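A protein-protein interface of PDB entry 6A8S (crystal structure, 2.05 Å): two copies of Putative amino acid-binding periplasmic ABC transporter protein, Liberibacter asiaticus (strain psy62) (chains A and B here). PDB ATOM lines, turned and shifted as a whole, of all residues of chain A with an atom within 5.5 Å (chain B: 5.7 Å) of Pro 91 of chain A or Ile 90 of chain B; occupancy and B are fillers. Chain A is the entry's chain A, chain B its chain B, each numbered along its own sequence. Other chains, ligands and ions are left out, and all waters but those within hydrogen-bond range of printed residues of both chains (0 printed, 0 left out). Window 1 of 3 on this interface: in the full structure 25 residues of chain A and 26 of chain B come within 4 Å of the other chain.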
ATOM      1  N   ILE A  78       3.208  -9.483  15.571  1.00  0.00           N
ATOM      2  CA  ILE A  78       2.648 -10.734  16.079  1.00  0.00           C
ATOM      3  C   ILE A  78       1.460 -10.408  16.965  1.00  0.00           C
ATOM      4  O   ILE A  78       1.566  -9.580  17.877  1.00  0.00           O
ATOM      5  CB  ILE A  78       3.713 -11.534  16.862  1.00  0.00           C
ATOM      6  CG1 ILE A  78       4.850 -11.994  15.943  1.00  0.00           C
ATOM      7  CG2 ILE A  78       3.081 -12.698  17.619  1.00  0.00           C
ATOM      8  CD1 ILE A  78       5.950 -12.832  16.652  1.00  0.00           C
ATOM      9  N   GLN A  83      -1.157 -15.488  15.241  1.00  0.00           N
ATOM     10  CA  GLN A  83      -0.502 -16.729  15.651  1.00  0.00           C
ATOM     11  C   GLN A  83      -1.474 -17.906  15.607  1.00  0.00           C
ATOM     12  O   GLN A  83      -1.058 -19.045  15.389  1.00  0.00           O
ATOM     13  CB  GLN A  83       0.115 -16.563  17.058  1.00  0.00           C
ATOM     14  CG  GLN A  83       1.557 -17.131  17.220  1.00  0.00           C
ATOM     15  CD  GLN A  83       2.422 -16.403  18.278  1.00  0.00           C
ATOM     16  OE1 GLN A  83       1.906 -15.830  19.243  1.00  0.00           O
ATOM     17  NE2 GLN A  83       3.745 -16.429  18.084  1.00  0.00           N
ATOM     18  N   SER A  89       7.893 -16.544  11.899  1.00  0.00           N
ATOM     19  CA  SER A  89       9.287 -16.783  12.213  1.00  0.00           C
ATOM     20  C   SER A  89       9.555 -16.323  13.646  1.00  0.00           C
ATOM     21  O   SER A  89       8.686 -15.761  14.322  1.00  0.00           O
ATOM     22  CB  SER A  89      10.190 -16.047  11.222  1.00  0.00           C
ATOM     23  OG  SER A  89      10.256 -14.656  11.502  1.00  0.00           O
ATOM     24  N   ILE A  90      10.763 -16.571  14.126  1.00  0.00           N
ATOM     25  CA  ILE A  90      11.159 -15.943  15.381  1.00  0.00           C
ATOM     26  C   ILE A  90      11.132 -14.434  15.144  1.00  0.00           C
ATOM     27  O   ILE A  90      11.409 -13.985  14.017  1.00  0.00           O
ATOM     28  CB  ILE A  90      12.535 -16.438  15.834  1.00  0.00           C
ATOM     29  CG1 ILE A  90      12.839 -15.960  17.253  1.00  0.00           C
ATOM     30  CG2 ILE A  90      13.594 -16.000  14.851  1.00  0.00           C
ATOM     31  CD1 ILE A  90      14.148 -16.462  17.796  1.00  0.00           C
ATOM     32  N   PRO A  91      10.772 -13.613  16.134  1.00  0.00           N
ATOM     33  CA  PRO A  91      10.811 -12.154  15.923  1.00  0.00           C
ATOM     34  C   PRO A  91      12.216 -11.710  15.539  1.00  0.00           C
ATOM     35  O   PRO A  91      13.200 -12.246  16.035  1.00  0.00           O
ATOM     36  CB  PRO A  91      10.386 -11.577  17.283  1.00  0.00           C
ATOM     37  CG  PRO A  91       9.626 -12.664  17.952  1.00  0.00           C
ATOM     38  CD  PRO A  91      10.186 -13.975  17.437  1.00  0.00           C
ATOM     39  N   TYR A  92      12.309 -10.752  14.613  1.00  0.00           N
ATOM     40  CA  TYR A  92      13.609 -10.245  14.184  1.00  0.00           C
ATOM     41  C   TYR A  92      13.785  -8.753  14.412  1.00  0.00           C
ATOM     42  O   TYR A  92      14.860  -8.227  14.122  1.00  0.00           O
ATOM     43  CB  TYR A  92      13.873 -10.563  12.702  1.00  0.00           C
ATOM     44  CG  TYR A  92      12.902  -9.949  11.705  1.00  0.00           C
ATOM     45  CD1 TYR A  92      13.008  -8.616  11.325  1.00  0.00           C
ATOM     46  CD2 TYR A  92      11.899 -10.712  11.127  1.00  0.00           C
ATOM     47  CE1 TYR A  92      12.129  -8.050  10.404  1.00  0.00           C
ATOM     48  CE2 TYR A  92      11.013 -10.159  10.200  1.00  0.00           C
ATOM     49  CZ  TYR A  92      11.142  -8.823   9.847  1.00  0.00           C
ATOM     50  OH  TYR A  92      10.284  -8.258   8.938  1.00  0.00           O
ATOM     51  N   ILE A  93      12.764  -8.066  14.910  1.00  0.00           N
ATOM     52  CA  ILE A  93      12.828  -6.651  15.251  1.00  0.00           C
ATOM     53  C   ILE A  93      11.629  -6.388  16.148  1.00  0.00           C
ATOM     54  O   ILE A  93      10.751  -7.246  16.284  1.00  0.00           O
ATOM     55  CB  ILE A  93      12.830  -5.753  13.999  1.00  0.00           C
ATOM     56  CG1 ILE A  93      13.226  -4.331  14.379  1.00  0.00           C
ATOM     57  CG2 ILE A  93      11.491  -5.769  13.338  1.00  0.00           C
ATOM     58  CD1 ILE A  93      14.222  -3.755  13.484  1.00  0.00           C
ATOM     59  N   ALA A 191       6.676  -7.417  19.095  1.00  0.00           N
ATOM     60  CA  ALA A 191       7.549  -8.266  18.303  1.00  0.00           C
ATOM     61  C   ALA A 191       7.072  -8.290  16.854  1.00  0.00           C
ATOM     62  O   ALA A 191       5.872  -8.330  16.583  1.00  0.00           O
ATOM     63  CB  ALA A 191       7.580  -9.676  18.885  1.00  0.00           C
ATOM     64  N   VAL A 192       8.019  -8.252  15.925  1.00  0.00           N
ATOM     65  CA  VAL A 192       7.734  -8.254  14.496  1.00  0.00           C
ATOM     66  C   VAL A 192       8.426  -9.457  13.873  1.00  0.00           C
ATOM     67  O   VAL A 192       9.571  -9.764  14.220  1.00  0.00           O
ATOM     68  CB  VAL A 192       8.208  -6.946  13.830  1.00  0.00           C
ATOM     69  CG1 VAL A 192       8.078  -7.030  12.312  1.00  0.00           C
ATOM     70  CG2 VAL A 192       7.399  -5.782  14.354  1.00  0.00           C
ATOM     71  N   ALA A 193       7.744 -10.126  12.943  1.00  0.00           N
ATOM     72  CA  ALA A 193       8.254 -11.371  12.387  1.00  0.00           C
ATOM     73  C   ALA A 193       7.874 -11.493  10.915  1.00  0.00           C
ATOM     74  O   ALA A 193       7.084 -10.704  10.385  1.00  0.00           O
ATOM     75  CB  ALA A 193       7.726 -12.566  13.182  1.00  0.00           C
ATOM     76  N   HIS A 215      22.372 -13.385  13.114  1.00  0.00           N
ATOM     77  CA  HIS A 215      22.719 -12.680  14.347  1.00  0.00           C
ATOM     78  C   HIS A 215      24.166 -12.951  14.738  1.00  0.00           C
ATOM     79  O   HIS A 215      24.923 -12.024  15.054  1.00  0.00           O
ATOM     80  CB  HIS A 215      21.792 -13.099  15.490  1.00  0.00           C
ATOM     81  CG  HIS A 215      20.519 -12.320  15.570  1.00  0.00           C
ATOM     82  ND1 HIS A 215      20.400 -11.156  16.301  1.00  0.00           N
ATOM     83  CD2 HIS A 215      19.298 -12.550  15.026  1.00  0.00           C
ATOM     84  CE1 HIS A 215      19.164 -10.698  16.196  1.00  0.00           C
ATOM     85  NE2 HIS A 215      18.476 -11.526  15.430  1.00  0.00           N
ATOM     86  N   VAL A 236      15.921  -7.286  18.849  1.00  0.00           N
ATOM     87  CA  VAL A 236      15.497  -8.533  19.466  1.00  0.00           C
ATOM     88  C   VAL A 236      16.752  -9.109  20.115  1.00  0.00           C
ATOM     89  O   VAL A 236      17.864  -8.673  19.785  1.00  0.00           O
ATOM     90  CB  VAL A 236      14.886  -9.504  18.443  1.00  0.00           C
ATOM     91  CG1 VAL A 236      13.527  -8.997  17.934  1.00  0.00           C
ATOM     92  CG2 VAL A 236      15.860  -9.755  17.305  1.00  0.00           C
ATOM     93  N   PHE B  88      11.303 -24.778  18.934  1.00  0.00           N
ATOM     94  CA  PHE B  88      11.425 -23.754  19.964  1.00  0.00           C
ATOM     95  C   PHE B  88      10.157 -22.917  19.989  1.00  0.00           C
ATOM     96  O   PHE B  88       9.600 -22.600  18.942  1.00  0.00           O
ATOM     97  CB  PHE B  88      12.619 -22.812  19.709  1.00  0.00           C
ATOM     98  CG  PHE B  88      13.940 -23.308  20.235  1.00  0.00           C
ATOM     99  CD1 PHE B  88      14.163 -23.437  21.596  1.00  0.00           C
ATOM    100  CD2 PHE B  88      14.972 -23.607  19.363  1.00  0.00           C
ATOM    101  CE1 PHE B  88      15.397 -23.879  22.079  1.00  0.00           C
ATOM    102  CE2 PHE B  88      16.200 -24.037  19.837  1.00  0.00           C
ATOM    103  CZ  PHE B  88      16.417 -24.165  21.201  1.00  0.00           C
ATOM    104  N   SER B  89       9.708 -22.550  21.185  1.00  0.00           N
ATOM    105  CA  SER B  89       8.738 -21.481  21.281  1.00  0.00           C
ATOM    106  C   SER B  89       9.382 -20.159  20.874  1.00  0.00           C
ATOM    107  O   SER B  89      10.584 -20.062  20.592  1.00  0.00           O
ATOM    108  CB  SER B  89       8.161 -21.367  22.696  1.00  0.00           C
ATOM    109  OG  SER B  89       9.077 -20.758  23.597  1.00  0.00           O
ATOM    110  N   ILE B  90       8.546 -19.138  20.805  1.00  0.00           N
ATOM    111  CA  ILE B  90       9.017 -17.768  20.711  1.00  0.00           C
ATOM    112  C   ILE B  90       9.872 -17.516  21.955  1.00  0.00           C
ATOM    113  O   ILE B  90       9.594 -18.106  23.014  1.00  0.00           O
ATOM    114  CB  ILE B  90       7.816 -16.819  20.589  1.00  0.00           C
ATOM    115  CG1 ILE B  90       8.247 -15.426  20.134  1.00  0.00           C
ATOM    116  CG2 ILE B  90       7.030 -16.793  21.911  1.00  0.00           C
ATOM    117  CD1 ILE B  90       7.100 -14.430  20.130  1.00  0.00           C
ATOM    118  N   PRO B  91      10.941 -16.714  21.892  1.00  0.00           N
ATOM    119  CA  PRO B  91      11.715 -16.460  23.120  1.00  0.00           C
ATOM    120  C   PRO B  91      10.842 -15.787  24.167  1.00  0.00           C
ATOM    121  O   PRO B  91       9.940 -15.019  23.838  1.00  0.00           O
ATOM    122  CB  PRO B  91      12.853 -15.537  22.655  1.00  0.00           C
ATOM    123  CG  PRO B  91      12.989 -15.790  21.206  1.00  0.00           C
ATOM    124  CD  PRO B  91      11.588 -16.127  20.704  1.00  0.00           C
ATOM    125  N   TYR B  92      11.078 -16.120  25.440  1.00  0.00           N
ATOM    126  CA  TYR B  92      10.392 -15.430  26.530  1.00  0.00           C
ATOM    127  C   TYR B  92      11.322 -14.727  27.517  1.00  0.00           C
ATOM    128  O   TYR B  92      10.830 -14.052  28.424  1.00  0.00           O
ATOM    129  CB  TYR B  92       9.474 -16.392  27.305  1.00  0.00           C
ATOM    130  CG  TYR B  92      10.181 -17.528  28.018  1.00  0.00           C
ATOM    131  CD1 TYR B  92      10.743 -17.351  29.283  1.00  0.00           C
ATOM    132  CD2 TYR B  92      10.280 -18.772  27.429  1.00  0.00           C
ATOM    133  CE1 TYR B  92      11.376 -18.396  29.942  1.00  0.00           C
ATOM    134  CE2 TYR B  92      10.925 -19.814  28.065  1.00  0.00           C
ATOM    135  CZ  TYR B  92      11.476 -19.620  29.309  1.00  0.00           C
ATOM    136  OH  TYR B  92      12.093 -20.673  29.908  1.00  0.00           O
ATOM    137  N   VAL B 192      16.243 -17.038  25.043  1.00  0.00           N
ATOM    138  CA  VAL B 192      15.934 -18.267  25.751  1.00  0.00           C
ATOM    139  C   VAL B 192      14.481 -18.615  25.479  1.00  0.00           C
ATOM    140  O   VAL B 192      13.635 -17.717  25.439  1.00  0.00           O
ATOM    141  CB  VAL B 192      16.208 -18.098  27.255  1.00  0.00           C
ATOM    142  CG1 VAL B 192      15.748 -19.307  27.999  1.00  0.00           C
ATOM    143  CG2 VAL B 192      17.688 -17.853  27.483  1.00  0.00           C
ATOM    144  N   ALA B 193      14.191 -19.904  25.262  1.00  0.00           N
ATOM    145  CA  ALA B 193      12.827 -20.314  24.930  1.00  0.00           C
ATOM    146  C   ALA B 193      12.550 -21.720  25.455  1.00  0.00           C
ATOM    147  O   ALA B 193      13.433 -22.391  25.990  1.00  0.00           O
ATOM    148  CB  ALA B 193      12.586 -20.248  23.422  1.00  0.00           C
ATOM    149  N   PHE B 194      11.288 -22.149  25.334  1.00  0.00           N
ATOM    150  CA  PHE B 194      10.925 -23.525  25.643  1.00  0.00           C
ATOM    151  C   PHE B 194      11.307 -24.389  24.453  1.00  0.00           C
ATOM    152  O   PHE B 194      11.053 -24.014  23.305  1.00  0.00           O
ATOM    153  CB  PHE B 194       9.423 -23.670  25.939  1.00  0.00           C
ATOM    154  CG  PHE B 194       8.948 -22.918  27.167  1.00  0.00           C
ATOM    155  CD1 PHE B 194       9.437 -23.224  28.426  1.00  0.00           C
ATOM    156  CD2 PHE B 194       7.991 -21.908  27.054  1.00  0.00           C
ATOM    157  CE1 PHE B 194       9.011 -22.524  29.551  1.00  0.00           C
ATOM    158  CE2 PHE B 194       7.553 -21.207  28.171  1.00  0.00           C
ATOM    159  CZ  PHE B 194       8.062 -21.510  29.424  1.00  0.00           C
ATOM    160  N   ASN B 208       3.046 -20.568  22.080  1.00  0.00           N
ATOM    161  CA  ASN B 208       3.297 -19.232  21.546  1.00  0.00           C
ATOM    162  C   ASN B 208       2.087 -18.323  21.705  1.00  0.00           C
ATOM    163  O   ASN B 208       2.231 -17.160  22.097  1.00  0.00           O
ATOM    164  CB  ASN B 208       3.718 -19.324  20.082  1.00  0.00           C
ATOM    165  CG  ASN B 208       5.130 -19.800  19.932  1.00  0.00           C
ATOM    166  OD1 ASN B 208       5.812 -20.030  20.930  1.00  0.00           O
ATOM    167  ND2 ASN B 208       5.591 -19.945  18.697  1.00  0.00           N
ATOM    168  N   LEU B 211       1.718 -17.506  25.410  1.00  0.00           N
ATOM    169  CA  LEU B 211       2.722 -16.543  25.861  1.00  0.00           C
ATOM    170  C   LEU B 211       2.395 -15.133  25.378  1.00  0.00           C
ATOM    171  O   LEU B 211       2.666 -14.148  26.076  1.00  0.00           O
ATOM    172  CB  LEU B 211       4.106 -16.950  25.374  1.00  0.00           C
ATOM    173  CG  LEU B 211       4.850 -18.113  26.035  1.00  0.00           C
ATOM    174  CD1 LEU B 211       6.105 -18.385  25.244  1.00  0.00           C
ATOM    175  CD2 LEU B 211       5.191 -17.804  27.496  1.00  0.00           C
ATOM    176  N   PRO B 237      10.664  -8.638  23.409  1.00  0.00           N
ATOM    177  CA  PRO B 237       9.567  -7.779  22.939  1.00  0.00           C
ATOM    178  C   PRO B 237       8.199  -8.270  23.402  1.00  0.00           C
ATOM    179  O   PRO B 237       7.958  -9.469  23.546  1.00  0.00           O
ATOM    180  CB  PRO B 237       9.688  -7.853  21.410  1.00  0.00           C
ATOM    181  CG  PRO B 237      11.100  -8.186  21.153  1.00  0.00           C
ATOM    182  CD  PRO B 237      11.559  -9.039  22.303  1.00  0.00           C
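The side-chain amide oxygen of Gln 83 of chain A lies close to the backbone carbonyl oxygen of Asn 208 of chain B (3.2 Å).
Of chain B, only Ile 90 (3.6 Å) comes within 4 Å of Pro 91 of chain A. Of the printed residues of chain A, Ile 90 of chain B touches Ile 78 (3.997 Å) and Pro 91 (3.6 Å). Printed residues of chain A within 4 Å of Pro 237 of chain B: Ala 191. Printed residues of chain B within 4 Å of Ala 191 of chain A: Pro 237. His 215 of chain A touches none of the printed residues of chain B. Ala 193 of chain A touches none of the printed residues of chain B. The nearest residue of chain B that does not touch Pro 91 of chain A is Pro 91 of chain B (4.2 Å).
The backbone NH (N) of Ile 90 of chain B is in hydrogen-bond range of the side-chain amide oxygen (OD1) of Asn 208 of chain B (2.9 Å). The backbone NH of Ile 78 of chain A is in hydrogen-bond range of the backbone carbonyl oxygen of Ala 191 of chain A.
Of the 11 printed residues of chain B, 4 touch a printed residue of chain A. Hydrophobic or aromatic side chains of chain B within 4 Å of the printed part of chain A: Ile 90, Pro 91 and Pro 237. Of the 12 printed residues of chain A, 5 touch a printed residue of chain B. Hydrophobic or aromatic side chains of chain A that line the printed part of chain B: Ile 78, Ile 90, Pro 91 and Ala 191.
Among the printed residues, merely in contact across the chains: Ile 78 of chain A with Ile 90 of chain B (3.997 Å), Ile 90 of chain A with Pro 91 of chain B (3.7 Å), Pro 91 of chain A with Ile 90 of chain B (3.6 Å) and Ala 191 of chain A with Pro 237 of chain B (3.8 Å).
Ile 90 of chain A touches Pro 91 of chain B, and with the chains exchanged Pro 91 of chain A touches Ile 90 of chain B. 6 positions are printed for both chains. Of the 5 pairs that touch across the chains among the printed residues, 2 have their exchanged pair printed and touching as well.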
